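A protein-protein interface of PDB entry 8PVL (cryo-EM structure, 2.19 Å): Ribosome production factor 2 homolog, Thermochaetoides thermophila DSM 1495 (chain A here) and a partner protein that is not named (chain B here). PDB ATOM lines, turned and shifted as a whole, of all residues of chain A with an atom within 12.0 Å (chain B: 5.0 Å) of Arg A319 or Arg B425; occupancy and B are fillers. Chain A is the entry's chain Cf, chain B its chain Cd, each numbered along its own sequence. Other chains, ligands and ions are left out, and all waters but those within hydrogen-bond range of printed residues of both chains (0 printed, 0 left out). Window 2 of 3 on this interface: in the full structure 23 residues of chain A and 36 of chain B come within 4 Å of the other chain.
The backbone carbonyl oxygen (O) of Gly A316 is in hydrogen-bond range of the guanidinium group (NH1) of Arg B425 (3.4 Å).
The side-chain amino group (NZ) of Lys A315 is in salt-bridge range of the side-chain carboxylate (OE1) of Glu B428 (3.0 Å).
The backbone carbonyl oxygen of Thr B426 is in hydrogen-bond range of the side-chain amino group of Lys A315 (3.4 Å).
The guanidinium group (NH1) of Arg A319 lies within hydrogen-bond range of the backbone carbonyl oxygen (O) of Leu A317 (2.7 Å).
A ring nitrogen (NE2) of His B422 sits at hydrogen-bond distance from a ring nitrogen (NE2) of His B421 (3.3 Å).
The backbone carbonyl oxygen (O) of His B422 sits at hydrogen-bond distance from the side-chain hydroxyl (OG1) of Thr B426 (2.7 Å).
Among the printed residues, merely in contact across the chains: Lys A315 with Arg B425, Gly A316 with His B422, Gly A316 with Thr B426, Leu A317 with His B422, Lys A318 with Arg B425 and Arg A319 with Arg B425.
Arg A319 touches just one residue of chain B: Arg B425.
Printed residues of chain A within 4 Å of Arg B425: Lys A315, Gly A316, Lys A318 and Arg A319.
No residue of chain A comes within 4 Å of His B421.
Glu B428 touches just one residue of chain A: Lys A315 (3.0 Å).
Of the printed residues of chain B, Lys A318 touches Arg B425.
Of the printed residues of chain B, Leu A317 touches His B422.
Of the printed residues of chain B, Gly A316 touches His B422, Arg B425 and Thr B426.
Of the printed residues of chain B, Lys A315 touches Arg B425 (3.9 Å), Thr B426 (3.4 Å) and Glu B428 (3.0 Å).
Arg A312 touches none of the printed residues of chain B.
Tyr B427 touches none of the printed residues of chain A.
The nearest printed residue of chain B that does not touch Arg A319 is His B421 (7.8 Å).
The nearest printed residue of chain B that does not touch Lys A318 is Thr B426 (7.0 Å).
Of the 10 printed residues of chain A, 5 touch a printed residue of chain B.
Printed residues of chain A that touch a printed residue of chain B: Lys A315, Gly A316, Leu A317, Lys A318 and Arg A319.
Of the 9 printed residues of chain B, 4 touch a printed residue of chain A.
Hydrophobic or aromatic side chains of chain B that line the printed part of chain A: His B422.
Along chain B the printed residues that touch a printed residue of chain A span positions 422 to 428.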
ATOM      1  N   GLN A 310       4.300  12.980  16.301  1.00  0.00           N
ATOM      2  CA  GLN A 310       4.922  11.938  15.500  1.00  0.00           C
ATOM      3  C   GLN A 310       6.391  11.848  15.885  1.00  0.00           C
ATOM      4  O   GLN A 310       7.114  12.849  15.824  1.00  0.00           O
ATOM      5  CB  GLN A 310       4.775  12.229  14.008  1.00  0.00           C
ATOM      6  CG  GLN A 310       3.360  12.094  13.481  1.00  0.00           C
ATOM      7  CD  GLN A 310       2.807  10.694  13.652  1.00  0.00           C
ATOM      8  OE1 GLN A 310       3.482   9.709  13.361  1.00  0.00           O
ATOM      9  NE2 GLN A 310       1.573  10.600  14.128  1.00  0.00           N
ATOM     10  N   THR A 311       6.829  10.663  16.289  1.00  0.00           N
ATOM     11  CA  THR A 311       8.230  10.472  16.613  1.00  0.00           C
ATOM     12  C   THR A 311       9.053  10.373  15.333  1.00  0.00           C
ATOM     13  O   THR A 311       8.524  10.161  14.240  1.00  0.00           O
ATOM     14  CB  THR A 311       8.422   9.224  17.475  1.00  0.00           C
ATOM     15  OG1 THR A 311       7.713   8.124  16.896  1.00  0.00           O
ATOM     16  CG2 THR A 311       7.887   9.472  18.871  1.00  0.00           C
ATOM     17  N   ARG A 312      10.365  10.547  15.480  1.00  0.00           N
ATOM     18  CA  ARG A 312      11.251  10.584  14.324  1.00  0.00           C
ATOM     19  C   ARG A 312      11.348   9.207  13.681  1.00  0.00           C
ATOM     20  O   ARG A 312      11.697   8.224  14.340  1.00  0.00           O
ATOM     21  CB  ARG A 312      12.635  11.078  14.735  1.00  0.00           C
ATOM     22  CG  ARG A 312      13.569  11.335  13.570  1.00  0.00           C
ATOM     23  CD  ARG A 312      14.802  12.110  14.004  1.00  0.00           C
ATOM     24  NE  ARG A 312      15.689  12.382  12.880  1.00  0.00           N
ATOM     25  CZ  ARG A 312      15.535  13.388  12.030  1.00  0.00           C
ATOM     26  NH1 ARG A 312      14.546  14.257  12.158  1.00  0.00           N
ATOM     27  NH2 ARG A 312      16.394  13.524  11.025  1.00  0.00           N
ATOM     28  N   LYS A 313      11.033   9.139  12.387  1.00  0.00           N
ATOM     29  CA  LYS A 313      11.056   7.882  11.640  1.00  0.00           C
ATOM     30  C   LYS A 313      12.509   7.540  11.332  1.00  0.00           C
ATOM     31  O   LYS A 313      13.042   7.823  10.257  1.00  0.00           O
ATOM     32  CB  LYS A 313      10.224   7.989  10.368  1.00  0.00           C
ATOM     33  CG  LYS A 313       8.843   8.601  10.551  1.00  0.00           C
ATOM     34  CD  LYS A 313       8.033   7.888  11.621  1.00  0.00           C
ATOM     35  CE  LYS A 313       6.732   8.620  11.892  1.00  0.00           C
ATOM     36  NZ  LYS A 313       6.149   8.252  13.205  1.00  0.00           N
ATOM     37  N   MET A 314      13.161   6.915  12.306  1.00  0.00           N
ATOM     38  CA  MET A 314      14.578   6.628  12.178  1.00  0.00           C
ATOM     39  C   MET A 314      14.814   5.387  11.318  1.00  0.00           C
ATOM     40  O   MET A 314      13.957   4.505  11.189  1.00  0.00           O
ATOM     41  CB  MET A 314      15.212   6.450  13.556  1.00  0.00           C
ATOM     42  CG  MET A 314      15.605   7.766  14.204  1.00  0.00           C
ATOM     43  SD  MET A 314      16.668   7.580  15.644  1.00  0.00           S
ATOM     44  CE  MET A 314      15.530   8.015  16.954  1.00  0.00           C
ATOM     45  N   LYS A 315      16.008   5.344  10.717  1.00  0.00           N
ATOM     46  CA  LYS A 315      16.398   4.223   9.867  1.00  0.00           C
ATOM     47  C   LYS A 315      16.506   2.927  10.660  1.00  0.00           C
ATOM     48  O   LYS A 315      16.168   1.856  10.145  1.00  0.00           O
ATOM     49  CB  LYS A 315      17.723   4.540   9.173  1.00  0.00           C
ATOM     50  CG  LYS A 315      18.186   3.501   8.169  1.00  0.00           C
ATOM     51  CD  LYS A 315      19.556   3.850   7.612  1.00  0.00           C
ATOM     52  CE  LYS A 315      19.935   2.935   6.461  1.00  0.00           C
ATOM     53  NZ  LYS A 315      21.345   3.135   6.031  1.00  0.00           N
ATOM     54  N   GLY A 316      16.958   3.004  11.911  1.00  0.00           N
ATOM     55  CA  GLY A 316      17.021   1.832  12.761  1.00  0.00           C
ATOM     56  C   GLY A 316      15.685   1.327  13.256  1.00  0.00           C
ATOM     57  O   GLY A 316      15.613   0.206  13.767  1.00  0.00           O
ATOM     58  N   LEU A 317      14.626   2.124  13.117  1.00  0.00           N
ATOM     59  CA  LEU A 317      13.280   1.694  13.461  1.00  0.00           C
ATOM     60  C   LEU A 317      12.456   1.294  12.246  1.00  0.00           C
ATOM     61  O   LEU A 317      11.513   0.510  12.393  1.00  0.00           O
ATOM     62  CB  LEU A 317      12.549   2.797  14.236  1.00  0.00           C
ATOM     63  CG  LEU A 317      13.252   3.294  15.502  1.00  0.00           C
ATOM     64  CD1 LEU A 317      12.608   4.569  16.018  1.00  0.00           C
ATOM     65  CD2 LEU A 317      13.254   2.218  16.573  1.00  0.00           C
ATOM     66  N   LYS A 318      12.779   1.811  11.061  1.00  0.00           N
ATOM     67  CA  LYS A 318      12.127   1.389   9.824  1.00  0.00           C
ATOM     68  C   LYS A 318      12.547  -0.043   9.516  1.00  0.00           C
ATOM     69  O   LYS A 318      13.713  -0.298   9.200  1.00  0.00           O
ATOM     70  CB  LYS A 318      12.487   2.314   8.664  1.00  0.00           C
ATOM     71  CG  LYS A 318      11.868   3.693   8.733  1.00  0.00           C
ATOM     72  CD  LYS A 318      12.367   4.562   7.593  1.00  0.00           C
ATOM     73  CE  LYS A 318      11.614   5.877   7.526  1.00  0.00           C
ATOM     74  NZ  LYS A 318      12.138   6.753   6.445  1.00  0.00           N
ATOM     75  N   ARG A 319      11.594  -0.969   9.590  1.00  0.00           N
ATOM     76  CA  ARG A 319      11.849  -2.396   9.391  1.00  0.00           C
ATOM     77  C   ARG A 319      12.298  -2.692   7.963  1.00  0.00           C
ATOM     78  O   ARG A 319      11.476  -2.940   7.082  1.00  0.00           O
ATOM     79  CB  ARG A 319      10.601  -3.241   9.714  1.00  0.00           C
ATOM     80  CG  ARG A 319      10.184  -3.361  11.194  1.00  0.00           C
ATOM     81  CD  ARG A 319       9.548  -2.098  11.763  1.00  0.00           C
ATOM     82  NE  ARG A 319       8.766  -1.392  10.754  1.00  0.00           N
ATOM     83  CZ  ARG A 319       8.465  -0.102  10.806  1.00  0.00           C
ATOM     84  NH1 ARG A 319       8.863   0.662  11.809  1.00  0.00           N
ATOM     85  NH2 ARG A 319       7.748   0.436   9.823  1.00  0.00           N
ATOM     86  N   HIS B 421      19.577  -5.120  17.386  1.00  0.00           N
ATOM     87  CA  HIS B 421      18.828  -5.094  16.135  1.00  0.00           C
ATOM     88  C   HIS B 421      18.659  -3.673  15.610  1.00  0.00           C
ATOM     89  O   HIS B 421      18.591  -3.473  14.394  1.00  0.00           O
ATOM     90  CB  HIS B 421      17.470  -5.782  16.309  1.00  0.00           C
ATOM     91  CG  HIS B 421      16.525  -5.063  17.221  1.00  0.00           C
ATOM     92  ND1 HIS B 421      16.753  -4.926  18.573  1.00  0.00           N
ATOM     93  CD2 HIS B 421      15.338  -4.460  16.976  1.00  0.00           C
ATOM     94  CE1 HIS B 421      15.751  -4.260  19.120  1.00  0.00           C
ATOM     95  NE2 HIS B 421      14.880  -3.966  18.173  1.00  0.00           N
ATOM     96  N   HIS B 422      18.634  -2.680  16.503  1.00  0.00           N
ATOM     97  CA  HIS B 422      18.609  -1.287  16.066  1.00  0.00           C
ATOM     98  C   HIS B 422      19.892  -0.909  15.331  1.00  0.00           C
ATOM     99  O   HIS B 422      19.840  -0.255  14.285  1.00  0.00           O
ATOM    100  CB  HIS B 422      18.385  -0.365  17.263  1.00  0.00           C
ATOM    101  CG  HIS B 422      16.997  -0.427  17.817  1.00  0.00           C
ATOM    102  ND1 HIS B 422      16.703  -0.100  19.123  1.00  0.00           N
ATOM    103  CD2 HIS B 422      15.822  -0.779  17.243  1.00  0.00           C
ATOM    104  CE1 HIS B 422      15.407  -0.247  19.330  1.00  0.00           C
ATOM    105  NE2 HIS B 422      14.849  -0.658  18.205  1.00  0.00           N
ATOM    106  N   MET B 423      21.049  -1.331  15.852  1.00  0.00           N
ATOM    107  CA  MET B 423      22.315  -1.060  15.176  1.00  0.00           C
ATOM    108  C   MET B 423      22.407  -1.815  13.854  1.00  0.00           C
ATOM    109  O   MET B 423      22.905  -1.275  12.854  1.00  0.00           O
ATOM    110  CB  MET B 423      23.485  -1.436  16.085  1.00  0.00           C
ATOM    111  CG  MET B 423      23.774  -0.410  17.158  1.00  0.00           C
ATOM    112  SD  MET B 423      24.509   1.130  16.581  1.00  0.00           S
ATOM    113  CE  MET B 423      26.241   0.721  16.620  1.00  0.00           C
ATOM    114  N   GLU B 424      21.933  -3.066  13.842  1.00  0.00           N
ATOM    115  CA  GLU B 424      21.948  -3.869  12.624  1.00  0.00           C
ATOM    116  C   GLU B 424      21.073  -3.253  11.542  1.00  0.00           C
ATOM    117  O   GLU B 424      21.453  -3.229  10.367  1.00  0.00           O
ATOM    118  CB  GLU B 424      21.494  -5.297  12.932  1.00  0.00           C
ATOM    119  CG  GLU B 424      22.496  -6.111  13.734  1.00  0.00           C
ATOM    120  CD  GLU B 424      21.939  -7.443  14.189  1.00  0.00           C
ATOM    121  OE1 GLU B 424      20.704  -7.622  14.145  1.00  0.00           O
ATOM    122  OE2 GLU B 424      22.737  -8.314  14.593  1.00  0.00           O
ATOM    123  N   ARG B 425      19.907  -2.734  11.920  1.00  0.00           N
ATOM    124  CA  ARG B 425      19.039  -2.070  10.960  1.00  0.00           C
ATOM    125  C   ARG B 425      19.583  -0.711  10.541  1.00  0.00           C
ATOM    126  O   ARG B 425      19.346  -0.279   9.407  1.00  0.00           O
ATOM    127  CB  ARG B 425      17.638  -1.921  11.549  1.00  0.00           C
ATOM    128  CG  ARG B 425      16.525  -2.044  10.537  1.00  0.00           C
ATOM    129  CD  ARG B 425      15.194  -2.289  11.223  1.00  0.00           C
ATOM    130  NE  ARG B 425      15.199  -3.488  12.051  1.00  0.00           N
ATOM    131  CZ  ARG B 425      14.521  -3.615  13.183  1.00  0.00           C
ATOM    132  NH1 ARG B 425      13.784  -2.625  13.660  1.00  0.00           N
ATOM    133  NH2 ARG B 425      14.582  -4.762  13.851  1.00  0.00           N
ATOM    134  N   THR B 426      20.295  -0.022  11.436  1.00  0.00           N
ATOM    135  CA  THR B 426      20.880   1.267  11.088  1.00  0.00           C
ATOM    136  C   THR B 426      21.984   1.115  10.049  1.00  0.00           C
ATOM    137  O   THR B 426      22.029   1.870   9.071  1.00  0.00           O
ATOM    138  CB  THR B 426      21.418   1.954  12.345  1.00  0.00           C
ATOM    139  OG1 THR B 426      20.339   2.209  13.252  1.00  0.00           O
ATOM    140  CG2 THR B 426      22.097   3.273  11.999  1.00  0.00           C
ATOM    141  N   TYR B 427      22.868   0.135  10.225  1.00  0.00           N
ATOM    142  CA  TYR B 427      24.040   0.029   9.365  1.00  0.00           C
ATOM    143  C   TYR B 427      23.981  -1.110   8.356  1.00  0.00           C
ATOM    144  O   TYR B 427      24.970  -1.319   7.643  1.00  0.00           O
ATOM    145  CB  TYR B 427      25.302  -0.095  10.223  1.00  0.00           C
ATOM    146  CG  TYR B 427      25.590   1.163  11.002  1.00  0.00           C
ATOM    147  CD1 TYR B 427      25.921   2.342  10.347  1.00  0.00           C
ATOM    148  CD2 TYR B 427      25.512   1.183  12.388  1.00  0.00           C
ATOM    149  CE1 TYR B 427      26.177   3.501  11.046  1.00  0.00           C
ATOM    150  CE2 TYR B 427      25.766   2.338  13.098  1.00  0.00           C
ATOM    151  CZ  TYR B 427      26.098   3.493  12.421  1.00  0.00           C
ATOM    152  OH  TYR B 427      26.354   4.649  13.117  1.00  0.00           O
ATOM    153  N   GLU B 428      22.853  -1.831   8.261  1.00  0.00           N
ATOM    154  CA  GLU B 428      22.657  -2.940   7.313  1.00  0.00           C
ATOM    155  C   GLU B 428      23.749  -3.999   7.450  1.00  0.00           C
ATOM    156  O   GLU B 428      24.231  -4.564   6.467  1.00  0.00           O
ATOM    157  CB  GLU B 428      22.568  -2.436   5.871  1.00  0.00           C
ATOM    158  CG  GLU B 428      21.173  -2.043   5.430  1.00  0.00           C
ATOM    159  CD  GLU B 428      20.953  -0.547   5.461  1.00  0.00           C
ATOM    160  OE1 GLU B 428      21.800   0.166   6.038  1.00  0.00           O
ATOM    161  OE2 GLU B 428      19.935  -0.082   4.907  1.00  0.00           O
ATOM    162  N   ARG B 430      25.440  -7.234  10.118  1.00  0.00           N
ATOM    163  CA  ARG B 430      25.193  -8.165  11.211  1.00  0.00           C
ATOM    164  C   ARG B 430      26.283  -9.224  11.239  1.00  0.00           C
ATOM    165  O   ARG B 430      26.983  -9.452  10.250  1.00  0.00           O
ATOM    166  CB  ARG B 430      23.817  -8.830  11.090  1.00  0.00           C
ATOM    167  CG  ARG B 430      23.589  -9.571   9.787  1.00  0.00           C
ATOM    168  CD  ARG B 430      22.105  -9.754   9.517  1.00  0.00           C
ATOM    169  NE  ARG B 430      21.332  -8.577   9.894  1.00  0.00           N
ATOM    170  CZ  ARG B 430      21.152  -7.516   9.119  1.00  0.00           C
ATOM    171  NH1 ARG B 430      21.668  -7.455   7.902  1.00  0.00           N
ATOM    172  NH2 ARG B 430      20.435  -6.493   9.574  1.00  0.00           N
